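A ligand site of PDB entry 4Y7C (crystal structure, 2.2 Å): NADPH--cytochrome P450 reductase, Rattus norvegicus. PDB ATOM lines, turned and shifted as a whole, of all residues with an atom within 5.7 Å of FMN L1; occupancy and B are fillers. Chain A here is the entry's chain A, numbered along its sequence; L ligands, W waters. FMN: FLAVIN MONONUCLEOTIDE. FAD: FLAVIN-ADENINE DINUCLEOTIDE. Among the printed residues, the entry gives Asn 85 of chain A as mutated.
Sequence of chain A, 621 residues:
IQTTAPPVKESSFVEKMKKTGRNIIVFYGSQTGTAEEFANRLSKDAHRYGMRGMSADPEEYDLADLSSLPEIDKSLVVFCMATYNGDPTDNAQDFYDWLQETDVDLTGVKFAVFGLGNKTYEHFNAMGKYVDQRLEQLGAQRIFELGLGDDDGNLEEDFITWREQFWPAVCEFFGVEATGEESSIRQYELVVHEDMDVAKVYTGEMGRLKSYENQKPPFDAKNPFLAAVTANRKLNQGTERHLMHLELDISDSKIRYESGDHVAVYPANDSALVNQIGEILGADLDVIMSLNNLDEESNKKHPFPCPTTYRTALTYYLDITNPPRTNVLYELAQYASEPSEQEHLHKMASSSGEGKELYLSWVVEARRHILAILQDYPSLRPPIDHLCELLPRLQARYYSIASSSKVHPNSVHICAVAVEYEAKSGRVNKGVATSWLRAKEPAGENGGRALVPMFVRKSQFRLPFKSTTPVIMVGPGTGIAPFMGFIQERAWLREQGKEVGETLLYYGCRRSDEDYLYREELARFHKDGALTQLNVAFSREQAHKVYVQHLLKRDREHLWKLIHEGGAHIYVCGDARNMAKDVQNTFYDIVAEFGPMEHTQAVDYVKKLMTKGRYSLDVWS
An oxygen (O2') of FMN L1 sits at hydrogen-bond distance from the backbone carbonyl oxygen of Thr 83 (2.7 Å).
The backbone NH of Asn 118 sits at hydrogen-bond distance from an oxygen (O2) of FMN L1 (3.1 Å).
O of Leu 116 is in hydrogen-bond range of O2' of FMN L1.
An oxygen (O2P) of FMN L1 is in hydrogen-bond range of the backbone NH (N) of Gln 31 (2.7 Å).
An oxygen (O3P) of FMN L1 sits at hydrogen-bond distance from the backbone NH (N) of Ala 35, at 2.7 Å.
N of Thr 32 lies within hydrogen-bond range of O2P of FMN L1 (3.0 Å).
The backbone NH (N) of Gly 86 is in hydrogen-bond range of an oxygen (O4) of FMN L1, at 2.8 Å.
OG1 of Thr 32 sits at hydrogen-bond distance from O1P of FMN L1 (2.5 Å).
The backbone NH (N) of Thr 34 sits at hydrogen-bond distance from an oxygen (O1P) of FMN L1 (3.0 Å).
N of Asn 125 is in hydrogen-bond range of O2 of FMN L1 (2.7 Å).
O of His 123 sits at hydrogen-bond distance from N3 of FMN L1 (2.9 Å).
O1P of FMN L1 is in hydrogen-bond range of OG1 of Thr 34, 2.7 Å away.
The backbone NH of Gly 33 is in hydrogen-bond range of an oxygen (O1P) of FMN L1 (3.4 Å).
The side-chain hydroxyl of Ser 30 lies within hydrogen-bond range of an oxygen (O3P) of FMN L1 (2.5 Å).
An oxygen (O3') of FMN L1 sits at hydrogen-bond distance from the side-chain carboxylate (OD2) of Asp 151, at 3.3 Å.
OH of Tyr 84 lies within hydrogen-bond range of O2P of FMN L1, at 2.6 Å.
N of Asn 85 is in hydrogen-bond range of N5 of FMN L1 (2.9 Å).
The backbone NH (N) of Thr 83 lies within hydrogen-bond range of an oxygen (O2') of FMN L1 (3.5 Å).
The backbone NH of Leu 116 lies close to the side-chain amide oxygen of Asn 125 (3.0 Å).
N of Ala 82 sits at hydrogen-bond distance from O of Gly 29, 3.0 Å away.
The side-chain hydroxyl (OG1) of Thr 83 is in hydrogen-bond range of the backbone NH (N) of Ala 126.
The side-chain hydroxyl (OG) of Ser 30 is in hydrogen-bond range of the backbone NH (N) of Gly 33, 2.8 Å away.
The side-chain hydroxyl of Ser 30 sits at hydrogen-bond distance from the backbone NH of Thr 34, 3.3 Å away.
N of Gly 117 lies within hydrogen-bond range of OD1 of Asn 125.
The backbone NH (N) of Thr 83 is in hydrogen-bond range of the backbone carbonyl oxygen (O) of Leu 116 (3.2 Å).
The side-chain hydroxyl (OG1) of Thr 32 sits at hydrogen-bond distance from the side-chain hydroxyl (OH) of Tyr 84, at 2.5 Å.
Water W4 bridges the side-chain hydroxyl of Thr 34 and an oxygen (O4') of FMN L1.
Water W3 lies within hydrogen-bond range of OH of Tyr 84 (3.3 Å), OG1 of Thr 32 (3.4 Å) and O3' of FMN L1 (3.5 Å).
Ala 82 touches FMN L1 (CB to O5', 3.4 Å).
Gly 117 touches FMN L1.
Tyr 121 touches FMN L1 (CE1 to N5, 3.4 Å).
Phe 124 touches FMN L1 (CA to O2, 3.2 Å).
Leu 155 touches FMN L1 (CD2 to O4', 3.5 Å).
Hydrophobic or aromatic side chains within 4 Å of FMN L1: Ala 35, Ala 82, Tyr 84, Leu 116, Tyr 121, Phe 124 and Leu 155.
The nearest printed residue that does not touch FMN L1 is Gly 29 (4.2 Å).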
ATOM      1  N   GLY A  29       0.662   3.371  -5.413  1.00  0.00           N
ATOM      2  CA  GLY A  29       1.183   3.115  -4.101  1.00  0.00           C
ATOM      3  C   GLY A  29       1.891   4.398  -3.756  1.00  0.00           C
ATOM      4  O   GLY A  29       2.993   4.667  -4.234  1.00  0.00           O
ATOM      5  N   SER A  30       1.244   5.193  -2.917  1.00  0.00           N
ATOM      6  CA  SER A  30       1.815   6.481  -2.515  1.00  0.00           C
ATOM      7  C   SER A  30       1.597   6.845  -1.048  1.00  0.00           C
ATOM      8  O   SER A  30       0.643   6.413  -0.417  1.00  0.00           O
ATOM      9  CB  SER A  30       1.205   7.558  -3.413  1.00  0.00           C
ATOM     10  OG  SER A  30       1.667   8.851  -3.098  1.00  0.00           O
ATOM     11  N   GLN A  31       2.516   7.656  -0.509  1.00  0.00           N
ATOM     12  CA  GLN A  31       2.412   8.126   0.870  1.00  0.00           C
ATOM     13  C   GLN A  31       2.511   9.650   0.919  1.00  0.00           C
ATOM     14  O   GLN A  31       1.955  10.296   1.805  1.00  0.00           O
ATOM     15  CB  GLN A  31       3.495   7.486   1.742  1.00  0.00           C
ATOM     16  CG  GLN A  31       3.259   6.004   2.007  1.00  0.00           C
ATOM     17  CD  GLN A  31       4.163   5.396   3.069  1.00  0.00           C
ATOM     18  OE1 GLN A  31       4.047   4.210   3.386  1.00  0.00           O
ATOM     19  NE2 GLN A  31       5.072   6.204   3.622  1.00  0.00           N
ATOM     20  N   THR A  32       3.204  10.229  -0.049  1.00  0.00           N
ATOM     21  CA  THR A  32       3.356  11.675  -0.120  1.00  0.00           C
ATOM     22  C   THR A  32       2.607  12.218  -1.342  1.00  0.00           C
ATOM     23  O   THR A  32       2.739  13.389  -1.720  1.00  0.00           O
ATOM     24  CB  THR A  32       4.854  12.062  -0.185  1.00  0.00           C
ATOM     25  OG1 THR A  32       5.639  10.869  -0.281  1.00  0.00           O
ATOM     26  CG2 THR A  32       5.269  12.819   1.070  1.00  0.00           C
ATOM     27  N   GLY A  33       1.804  11.357  -1.960  1.00  0.00           N
ATOM     28  CA  GLY A  33       1.019  11.763  -3.106  1.00  0.00           C
ATOM     29  C   GLY A  33       1.687  11.816  -4.466  1.00  0.00           C
ATOM     30  O   GLY A  33       1.014  12.137  -5.445  1.00  0.00           O
ATOM     31  N   THR A  34       2.981  11.517  -4.551  1.00  0.00           N
ATOM     32  CA  THR A  34       3.667  11.571  -5.847  1.00  0.00           C
ATOM     33  C   THR A  34       3.201  10.509  -6.840  1.00  0.00           C
ATOM     34  O   THR A  34       2.971  10.805  -8.011  1.00  0.00           O
ATOM     35  CB  THR A  34       5.198  11.448  -5.676  1.00  0.00           C
ATOM     36  OG1 THR A  34       5.656  12.350  -4.661  1.00  0.00           O
ATOM     37  CG2 THR A  34       5.904  11.803  -6.991  1.00  0.00           C
ATOM     38  N   ALA A  35       3.060   9.262  -6.375  1.00  0.00           N
ATOM     39  CA  ALA A  35       2.617   8.153  -7.232  1.00  0.00           C
ATOM     40  C   ALA A  35       1.147   8.317  -7.567  1.00  0.00           C
ATOM     41  O   ALA A  35       0.676   7.878  -8.610  1.00  0.00           O
ATOM     42  CB  ALA A  35       2.842   6.812  -6.521  1.00  0.00           C
ATOM     43  N   GLU A  36       0.407   8.956  -6.662  1.00  0.00           N
ATOM     44  CA  GLU A  36      -1.001   9.187  -6.884  1.00  0.00           C
ATOM     45  C   GLU A  36      -1.184  10.147  -8.063  1.00  0.00           C
ATOM     46  O   GLU A  36      -2.040   9.936  -8.907  1.00  0.00           O
ATOM     47  CB  GLU A  36      -1.646   9.779  -5.621  1.00  0.00           C
ATOM     48  CG  GLU A  36      -3.146   9.720  -5.636  1.00  0.00           C
ATOM     49  CD  GLU A  36      -3.765  10.392  -4.422  1.00  0.00           C
ATOM     50  OE1 GLU A  36      -3.167  10.306  -3.324  1.00  0.00           O
ATOM     51  OE2 GLU A  36      -4.835  11.001  -4.582  1.00  0.00           O
ATOM     52  N   ALA A  82       5.594   3.525  -5.072  1.00  0.00           N
ATOM     53  CA  ALA A  82       6.716   4.110  -4.362  1.00  0.00           C
ATOM     54  C   ALA A  82       7.212   3.066  -3.373  1.00  0.00           C
ATOM     55  O   ALA A  82       6.479   2.133  -3.005  1.00  0.00           O
ATOM     56  CB  ALA A  82       6.275   5.361  -3.613  1.00  0.00           C
ATOM     57  N   THR A  83       8.460   3.212  -2.937  1.00  0.00           N
ATOM     58  CA  THR A  83       9.072   2.308  -1.973  1.00  0.00           C
ATOM     59  C   THR A  83       9.474   3.079  -0.730  1.00  0.00           C
ATOM     60  O   THR A  83       9.958   4.210  -0.815  1.00  0.00           O
ATOM     61  CB  THR A  83      10.353   1.637  -2.518  1.00  0.00           C
ATOM     62  OG1 THR A  83      10.030   0.852  -3.662  1.00  0.00           O
ATOM     63  CG2 THR A  83      10.977   0.747  -1.450  1.00  0.00           C
ATOM     64  N   TYR A  84       9.267   2.477   0.434  1.00  0.00           N
ATOM     65  CA  TYR A  84       9.648   3.102   1.688  1.00  0.00           C
ATOM     66  C   TYR A  84      10.366   2.101   2.579  1.00  0.00           C
ATOM     67  O   TYR A  84       9.760   1.121   3.041  1.00  0.00           O
ATOM     68  CB  TYR A  84       8.428   3.681   2.418  1.00  0.00           C
ATOM     69  CG  TYR A  84       7.972   5.019   1.861  1.00  0.00           C
ATOM     70  CD1 TYR A  84       7.121   5.090   0.750  1.00  0.00           C
ATOM     71  CD2 TYR A  84       8.389   6.213   2.446  1.00  0.00           C
ATOM     72  CE1 TYR A  84       6.706   6.318   0.239  1.00  0.00           C
ATOM     73  CE2 TYR A  84       7.984   7.444   1.935  1.00  0.00           C
ATOM     74  CZ  TYR A  84       7.148   7.495   0.828  1.00  0.00           C
ATOM     75  OH  TYR A  84       6.732   8.719   0.345  1.00  0.00           O
ATOM     76  N   ASN A  85      11.653   2.347   2.817  1.00  0.00           N
ATOM     77  CA  ASN A  85      12.478   1.483   3.647  1.00  0.00           C
ATOM     78  C   ASN A  85      12.444   0.058   3.099  1.00  0.00           C
ATOM     79  O   ASN A  85      12.259  -0.902   3.850  1.00  0.00           O
ATOM     80  CB  ASN A  85      11.983   1.503   5.101  1.00  0.00           C
ATOM     81  CG  ASN A  85      11.766   2.915   5.622  1.00  0.00           C
ATOM     82  OD1 ASN A  85      12.655   3.763   5.564  1.00  0.00           O
ATOM     83  ND2 ASN A  85      10.564   3.160   6.144  1.00  0.00           N
ATOM     84  N   GLY A  86      12.603  -0.058   1.783  1.00  0.00           N
ATOM     85  CA  GLY A  86      12.588  -1.355   1.150  1.00  0.00           C
ATOM     86  C   GLY A  86      11.236  -2.042   1.179  1.00  0.00           C
ATOM     87  O   GLY A  86      11.109  -3.193   0.756  1.00  0.00           O
ATOM     88  N   ASP A  87      10.219  -1.351   1.687  1.00  0.00           N
ATOM     89  CA  ASP A  87       8.881  -1.920   1.773  1.00  0.00           C
ATOM     90  C   ASP A  87       7.854  -1.165   0.943  1.00  0.00           C
ATOM     91  O   ASP A  87       8.160  -0.103   0.391  1.00  0.00           O
ATOM     92  CB  ASP A  87       8.394  -1.935   3.228  1.00  0.00           C
ATOM     93  CG  ASP A  87       9.176  -2.897   4.105  1.00  0.00           C
ATOM     94  OD1 ASP A  87       9.377  -4.057   3.678  1.00  0.00           O
ATOM     95  OD2 ASP A  87       9.560  -2.497   5.219  1.00  0.00           O
ATOM     96  N   THR A  89       4.261   0.983   0.206  1.00  0.00           N
ATOM     97  CA  THR A  89       3.649   2.087   0.912  1.00  0.00           C
ATOM     98  C   THR A  89       2.560   1.468   1.782  1.00  0.00           C
ATOM     99  O   THR A  89       2.099   0.360   1.499  1.00  0.00           O
ATOM    100  CB  THR A  89       3.012   3.112  -0.067  1.00  0.00           C
ATOM    101  OG1 THR A  89       2.104   2.427  -0.950  1.00  0.00           O
ATOM    102  CG2 THR A  89       4.085   3.800  -0.889  1.00  0.00           C
ATOM    103  N   LEU A 116       8.586   4.499  -8.110  1.00  0.00           N
ATOM    104  CA  LEU A 116       9.128   5.751  -7.578  1.00  0.00           C
ATOM    105  C   LEU A 116      10.100   5.391  -6.465  1.00  0.00           C
ATOM    106  O   LEU A 116       9.720   4.774  -5.472  1.00  0.00           O
ATOM    107  CB  LEU A 116       8.015   6.637  -7.002  1.00  0.00           C
ATOM    108  CG  LEU A 116       7.038   7.329  -7.964  1.00  0.00           C
ATOM    109  CD1 LEU A 116       6.032   6.341  -8.485  1.00  0.00           C
ATOM    110  CD2 LEU A 116       6.327   8.459  -7.233  1.00  0.00           C
ATOM    111  N   GLY A 117      11.359   5.768  -6.643  1.00  0.00           N
ATOM    112  CA  GLY A 117      12.357   5.453  -5.630  1.00  0.00           C
ATOM    113  C   GLY A 117      13.401   6.544  -5.493  1.00  0.00           C
ATOM    114  O   GLY A 117      13.225   7.657  -6.013  1.00  0.00           O
ATOM    115  N   ASN A 118      14.488   6.222  -4.802  1.00  0.00           N
ATOM    116  CA  ASN A 118      15.580   7.163  -4.590  1.00  0.00           C
ATOM    117  C   ASN A 118      16.887   6.364  -4.475  1.00  0.00           C
ATOM    118  O   ASN A 118      17.096   5.669  -3.487  1.00  0.00           O
ATOM    119  CB  ASN A 118      15.341   7.964  -3.307  1.00  0.00           C
ATOM    120  CG  ASN A 118      16.346   9.082  -3.122  1.00  0.00           C
ATOM    121  OD1 ASN A 118      17.552   8.861  -3.217  1.00  0.00           O
ATOM    122  ND2 ASN A 118      15.847  10.286  -2.856  1.00  0.00           N
ATOM    123  N   LYS A 119      17.749   6.486  -5.476  1.00  0.00           N
ATOM    124  CA  LYS A 119      19.011   5.735  -5.489  1.00  0.00           C
ATOM    125  C   LYS A 119      19.842   5.816  -4.216  1.00  0.00           C
ATOM    126  O   LYS A 119      20.728   4.998  -4.008  1.00  0.00           O
ATOM    127  CB  LYS A 119      19.863   6.146  -6.692  1.00  0.00           C
ATOM    128  CG  LYS A 119      19.397   5.552  -8.020  1.00  0.00           C
ATOM    129  CD  LYS A 119      20.518   5.619  -9.056  1.00  0.00           C
ATOM    130  CE  LYS A 119      20.146   4.909 -10.361  1.00  0.00           C
ATOM    131  NZ  LYS A 119      19.069   5.636 -11.096  1.00  0.00           N
ATOM    132  N   TYR A 121      19.426   4.739  -1.558  1.00  0.00           N
ATOM    133  CA  TYR A 121      18.899   3.681  -0.707  1.00  0.00           C
ATOM    134  C   TYR A 121      19.371   2.322  -1.215  1.00  0.00           C
ATOM    135  O   TYR A 121      19.533   2.123  -2.425  1.00  0.00           O
ATOM    136  CB  TYR A 121      17.375   3.726  -0.675  1.00  0.00           C
ATOM    137  CG  TYR A 121      16.807   4.893   0.107  1.00  0.00           C
ATOM    138  CD1 TYR A 121      16.559   4.783   1.477  1.00  0.00           C
ATOM    139  CD2 TYR A 121      16.523   6.103  -0.513  1.00  0.00           C
ATOM    140  CE1 TYR A 121      16.046   5.846   2.207  1.00  0.00           C
ATOM    141  CE2 TYR A 121      16.006   7.188   0.213  1.00  0.00           C
ATOM    142  CZ  TYR A 121      15.774   7.055   1.565  1.00  0.00           C
ATOM    143  OH  TYR A 121      15.254   8.104   2.278  1.00  0.00           O
ATOM    144  N   HIS A 123      17.741  -0.446  -1.032  1.00  0.00           N
ATOM    145  CA  HIS A 123      16.590  -1.055  -1.683  1.00  0.00           C
ATOM    146  C   HIS A 123      15.891  -0.078  -2.628  1.00  0.00           C
ATOM    147  O   HIS A 123      14.747   0.305  -2.412  1.00  0.00           O
ATOM    148  CB  HIS A 123      15.598  -1.545  -0.625  1.00  0.00           C
ATOM    149  CG  HIS A 123      16.214  -2.478   0.385  1.00  0.00           C
ATOM    150  ND1 HIS A 123      16.741  -3.698   0.037  1.00  0.00           N
ATOM    151  CD2 HIS A 123      16.378  -2.354   1.721  1.00  0.00           C
ATOM    152  CE1 HIS A 123      17.209  -4.287   1.126  1.00  0.00           C
ATOM    153  NE2 HIS A 123      17.003  -3.488   2.158  1.00  0.00           N
ATOM    154  N   PHE A 124      16.598   0.306  -3.680  1.00  0.00           N
ATOM    155  CA  PHE A 124      16.093   1.245  -4.672  1.00  0.00           C
ATOM    156  C   PHE A 124      14.919   0.689  -5.486  1.00  0.00           C
ATOM    157  O   PHE A 124      15.081  -0.253  -6.257  1.00  0.00           O
ATOM    158  CB  PHE A 124      17.234   1.631  -5.617  1.00  0.00           C
ATOM    159  CG  PHE A 124      16.803   2.457  -6.801  1.00  0.00           C
ATOM    160  CD1 PHE A 124      16.196   3.701  -6.608  1.00  0.00           C
ATOM    161  CD2 PHE A 124      17.011   2.004  -8.096  1.00  0.00           C
ATOM    162  CE1 PHE A 124      15.811   4.478  -7.699  1.00  0.00           C
ATOM    163  CE2 PHE A 124      16.618   2.773  -9.196  1.00  0.00           C
ATOM    164  CZ  PHE A 124      16.023   4.011  -8.997  1.00  0.00           C
ATOM    165  N   ASN A 125      13.741   1.290  -5.304  1.00  0.00           N
ATOM    166  CA  ASN A 125      12.547   0.860  -6.025  1.00  0.00           C
ATOM    167  C   ASN A 125      12.166  -0.603  -5.802  1.00  0.00           C
ATOM    168  O   ASN A 125      11.630  -1.254  -6.710  1.00  0.00           O
ATOM    169  CB  ASN A 125      12.722   1.109  -7.530  1.00  0.00           C
ATOM    170  CG  ASN A 125      12.221   2.480  -7.946  1.00  0.00           C
ATOM    171  OD1 ASN A 125      11.114   2.897  -7.586  1.00  0.00           O
ATOM    172  ND2 ASN A 125      13.039   3.198  -8.715  1.00  0.00           N
ATOM    173  N   ALA A 126      12.420  -1.117  -4.610  1.00  0.00           N
ATOM    174  CA  ALA A 126      12.121  -2.506  -4.287  1.00  0.00           C
ATOM    175  C   ALA A 126      10.684  -2.891  -4.630  1.00  0.00           C
ATOM    176  O   ALA A 126      10.442  -3.944  -5.216  1.00  0.00           O
ATOM    177  CB  ALA A 126      12.378  -2.760  -2.806  1.00  0.00           C
ATOM    178  N   ASP A 151      14.186   9.758  -7.439  1.00  0.00           N
ATOM    179  CA  ASP A 151      13.929  11.043  -6.826  1.00  0.00           C
ATOM    180  C   ASP A 151      15.181  11.804  -6.385  1.00  0.00           C
ATOM    181  O   ASP A 151      15.066  12.915  -5.857  1.00  0.00           O
ATOM    182  CB  ASP A 151      12.970  10.853  -5.637  1.00  0.00           C
ATOM    183  CG  ASP A 151      12.387  12.160  -5.139  1.00  0.00           C
ATOM    184  OD1 ASP A 151      12.003  13.017  -5.965  1.00  0.00           O
ATOM    185  OD2 ASP A 151      12.300  12.334  -3.897  1.00  0.00           O
ATOM    186  N   LEU A 155      12.748  12.851 -10.469  1.00  0.00           N
ATOM    187  CA  LEU A 155      11.678  11.899 -10.683  1.00  0.00           C
ATOM    188  C   LEU A 155      10.731  12.338 -11.796  1.00  0.00           C
ATOM    189  O   LEU A 155      10.396  11.550 -12.682  1.00  0.00           O
ATOM    190  CB  LEU A 155      10.906  11.715  -9.375  1.00  0.00           C
ATOM    191  CG  LEU A 155       9.704  10.769  -9.396  1.00  0.00           C
ATOM    192  CD1 LEU A 155      10.178   9.357  -9.720  1.00  0.00           C
ATOM    193  CD2 LEU A 155       8.984  10.815  -8.041  1.00  0.00           C
ATOM    194  N   ARG A 457       2.708   7.841  13.849  1.00  0.00           N
ATOM    195  CA  ARG A 457       2.902   6.734  12.929  1.00  0.00           C
ATOM    196  C   ARG A 457       3.977   5.852  13.536  1.00  0.00           C
ATOM    197  O   ARG A 457       5.103   6.287  13.748  1.00  0.00           O
ATOM    198  CB  ARG A 457       3.373   7.202  11.551  1.00  0.00           C
ATOM    199  CG  ARG A 457       3.509   6.044  10.557  1.00  0.00           C
ATOM    200  CD  ARG A 457       4.013   6.494   9.198  1.00  0.00           C
ATOM    201  NE  ARG A 457       5.363   7.063   9.299  1.00  0.00           N
ATOM    202  CZ  ARG A 457       5.992   7.664   8.292  1.00  0.00           C
ATOM    203  NH1 ARG A 457       5.411   7.784   7.099  1.00  0.00           N
ATOM    204  NH2 ARG A 457       7.223   8.142   8.469  1.00  0.00           N
ATOM    205  N   VAL A 619      16.681   8.106   8.669  1.00  0.00           N
ATOM    206  CA  VAL A 619      17.262   9.180   7.879  1.00  0.00           C
ATOM    207  C   VAL A 619      16.276   9.822   6.900  1.00  0.00           C
ATOM    208  O   VAL A 619      15.275   9.225   6.505  1.00  0.00           O
ATOM    209  CB  VAL A 619      18.492   8.663   7.095  1.00  0.00           C
ATOM    210  CG1 VAL A 619      19.617   8.341   8.051  1.00  0.00           C
ATOM    211  CG2 VAL A 619      18.126   7.421   6.294  1.00  0.00           C
HETATM  212  N1  FMN L   1      13.135   4.943  -2.198  1.00  0.00           N
HETATM  213  C2  FMN L   1      13.637   3.731  -2.495  1.00  0.00           C
HETATM  214  O2  FMN L   1      13.895   3.403  -3.646  1.00  0.00           O
HETATM  215  N3  FMN L   1      13.855   2.879  -1.433  1.00  0.00           N
HETATM  216  C4  FMN L   1      13.615   3.124  -0.074  1.00  0.00           C
HETATM  217  O4  FMN L   1      13.894   2.199   0.682  1.00  0.00           O
HETATM  218  C4A FMN L   1      13.095   4.416   0.250  1.00  0.00           C
HETATM  219  N5  FMN L   1      12.844   4.708   1.625  1.00  0.00           N
HETATM  220  C5A FMN L   1      12.340   5.999   1.842  1.00  0.00           C
HETATM  221  C6  FMN L   1      12.090   6.333   3.224  1.00  0.00           C
HETATM  222  C7  FMN L   1      11.580   7.612   3.596  1.00  0.00           C
HETATM  223  C7M FMN L   1      11.366   7.842   5.118  1.00  0.00           C
HETATM  224  C8  FMN L   1      11.292   8.651   2.552  1.00  0.00           C
HETATM  225  C8M FMN L   1      10.801   9.920   2.786  1.00  0.00           C
HETATM  226  C9  FMN L   1      11.526   8.326   1.221  1.00  0.00           C
HETATM  227  C9A FMN L   1      12.054   7.019   0.823  1.00  0.00           C
HETATM  228  N10 FMN L   1      12.328   6.619  -0.570  1.00  0.00           N
HETATM  229  C10 FMN L   1      12.866   5.283  -0.873  1.00  0.00           C
HETATM  230  C1' FMN L   1      12.063   7.553  -1.661  1.00  0.00           C
HETATM  231  C2' FMN L   1      10.591   7.478  -2.188  1.00  0.00           C
HETATM  232  O2' FMN L   1      10.339   6.110  -2.707  1.00  0.00           O
HETATM  233  C3' FMN L   1      10.385   8.480  -3.302  1.00  0.00           C
HETATM  234  O3' FMN L   1      10.636   9.795  -2.735  1.00  0.00           O
HETATM  235  C4' FMN L   1       8.909   8.378  -3.848  1.00  0.00           C
HETATM  236  O4' FMN L   1       8.946   9.379  -4.902  1.00  0.00           O
HETATM  237  C5' FMN L   1       7.833   8.853  -2.883  1.00  0.00           C
HETATM  238  O5' FMN L   1       6.467   8.721  -3.461  1.00  0.00           O
HETATM  239  P   FMN L   1       5.098   9.146  -2.788  1.00  0.00           P
HETATM  240  O1P FMN L   1       5.062  10.614  -2.664  1.00  0.00           O
HETATM  241  O2P FMN L   1       4.987   8.251  -1.502  1.00  0.00           O
HETATM  242  O3P FMN L   1       4.059   8.703  -3.925  1.00  0.00           O
HETATM  243  PA  FAD L   2       8.998  22.381   3.034  1.00  0.00           P
HETATM  244  O1A FAD L   2       8.111  23.516   2.731  1.00  0.00           O
HETATM  245  O2A FAD L   2       8.447  21.003   3.019  1.00  0.00           O
HETATM  246  O5B FAD L   2      10.270  22.442   2.056  1.00  0.00           O
HETATM  247  C5B FAD L   2      11.203  21.361   2.010  1.00  0.00           C
HETATM  248  C4B FAD L   2      12.038  21.480   0.735  1.00  0.00           C
HETATM  249  O4B FAD L   2      12.741  22.732   0.695  1.00  0.00           O
HETATM  250  C3B FAD L   2      13.178  20.480   0.735  1.00  0.00           C
HETATM  251  O3B FAD L   2      12.657  19.190   0.369  1.00  0.00           O
HETATM  252  C2B FAD L   2      13.965  21.046  -0.427  1.00  0.00           C
HETATM  253  O2B FAD L   2      13.363  20.642  -1.667  1.00  0.00           O
HETATM  254  C1B FAD L   2      13.827  22.546  -0.235  1.00  0.00           C
HETATM  255  N9A FAD L   2      15.024  23.127   0.419  1.00  0.00           N
HETATM  256  C8A FAD L   2      15.328  23.094   1.867  1.00  0.00           C
HETATM  257  N7A FAD L   2      16.574  23.880   1.896  1.00  0.00           N
HETATM  258  C5A FAD L   2      16.900  24.229   0.647  1.00  0.00           C
HETATM  259  C6A FAD L   2      17.930  24.929   0.214  1.00  0.00           C
HETATM  260  N6A FAD L   2      18.776  25.367   1.133  1.00  0.00           N
HETATM  261  N1A FAD L   2      18.167  25.130  -1.097  1.00  0.00           N
HETATM  262  C2A FAD L   2      17.308  24.566  -2.030  1.00  0.00           C
HETATM  263  N3A FAD L   2      16.235  23.811  -1.543  1.00  0.00           N
HETATM  264  C4A FAD L   2      16.048  23.663  -0.222  1.00  0.00           C
HETATM  265  N1  FAD L   2      13.107  17.325  10.236  1.00  0.00           N
HETATM  266  C2  FAD L   2      13.502  17.839  11.471  1.00  0.00           C
HETATM  267  O2  FAD L   2      13.923  18.989  11.546  1.00  0.00           O
HETATM  268  N3  FAD L   2      13.473  17.024  12.607  1.00  0.00           N
HETATM  269  C4  FAD L   2      13.063  15.686  12.493  1.00  0.00           C
HETATM  270  O4  FAD L   2      12.984  14.989  13.513  1.00  0.00           O
HETATM  271  C4X FAD L   2      12.677  15.174  11.259  1.00  0.00           C
HETATM  272  N5  FAD L   2      12.446  13.863  11.123  1.00  0.00           N
HETATM  273  C5X FAD L   2      12.053  13.377   9.943  1.00  0.00           C
HETATM  274  C6  FAD L   2      11.715  12.033   9.822  1.00  0.00           C
HETATM  275  C7  FAD L   2      11.232  11.539   8.618  1.00  0.00           C
HETATM  276  C7M FAD L   2      10.751  10.238   8.538  1.00  0.00           C
HETATM  277  C8  FAD L   2      11.109  12.389   7.515  1.00  0.00           C
HETATM  278  C8M FAD L   2      10.646  11.901   6.298  1.00  0.00           C
HETATM  279  C9  FAD L   2      11.437  13.730   7.636  1.00  0.00           C
HETATM  280  C9A FAD L   2      11.897  14.232   8.855  1.00  0.00           C
HETATM  281  N10 FAD L   2      12.157  15.548   8.992  1.00  0.00           N
HETATM  282  C10 FAD L   2      12.696  15.984  10.136  1.00  0.00           C
HETATM  283  C1' FAD L   2      11.987  16.481   7.859  1.00  0.00           C
HETATM  284  C2' FAD L   2      10.581  17.087   7.895  1.00  0.00           C
HETATM  285  O2' FAD L   2       9.620  16.059   7.670  1.00  0.00           O
HETATM  286  C3' FAD L   2      10.414  18.185   6.834  1.00  0.00           C
HETATM  287  O3' FAD L   2      10.805  17.687   5.555  1.00  0.00           O
HETATM  288  C4' FAD L   2      11.267  19.400   7.205  1.00  0.00           C
HETATM  289  O4' FAD L   2      10.971  19.819   8.544  1.00  0.00           O
HETATM  290  C5' FAD L   2      10.985  20.541   6.215  1.00  0.00           C
HETATM  291  O5' FAD L   2       9.562  20.719   6.113  1.00  0.00           O
HETATM  292  P   FAD L   2       8.926  22.168   5.838  1.00  0.00           P
HETATM  293  O1P FAD L   2       9.325  23.091   6.914  1.00  0.00           O
HETATM  294  O2P FAD L   2       7.486  21.977   5.557  1.00  0.00           O
HETATM  295  O3P FAD L   2       9.662  22.632   4.478  1.00  0.00           O
HETATM  296  O   HOH W   1      15.911   0.869   3.183  1.00  0.00           O
HETATM  297  O   HOH W   2       8.211   8.150   5.799  1.00  0.00           O
HETATM  298  O   HOH W   3       9.020  11.046   0.102  1.00  0.00           O
HETATM  299  O   HOH W   4       8.270  12.334  -4.293  1.00  0.00           O
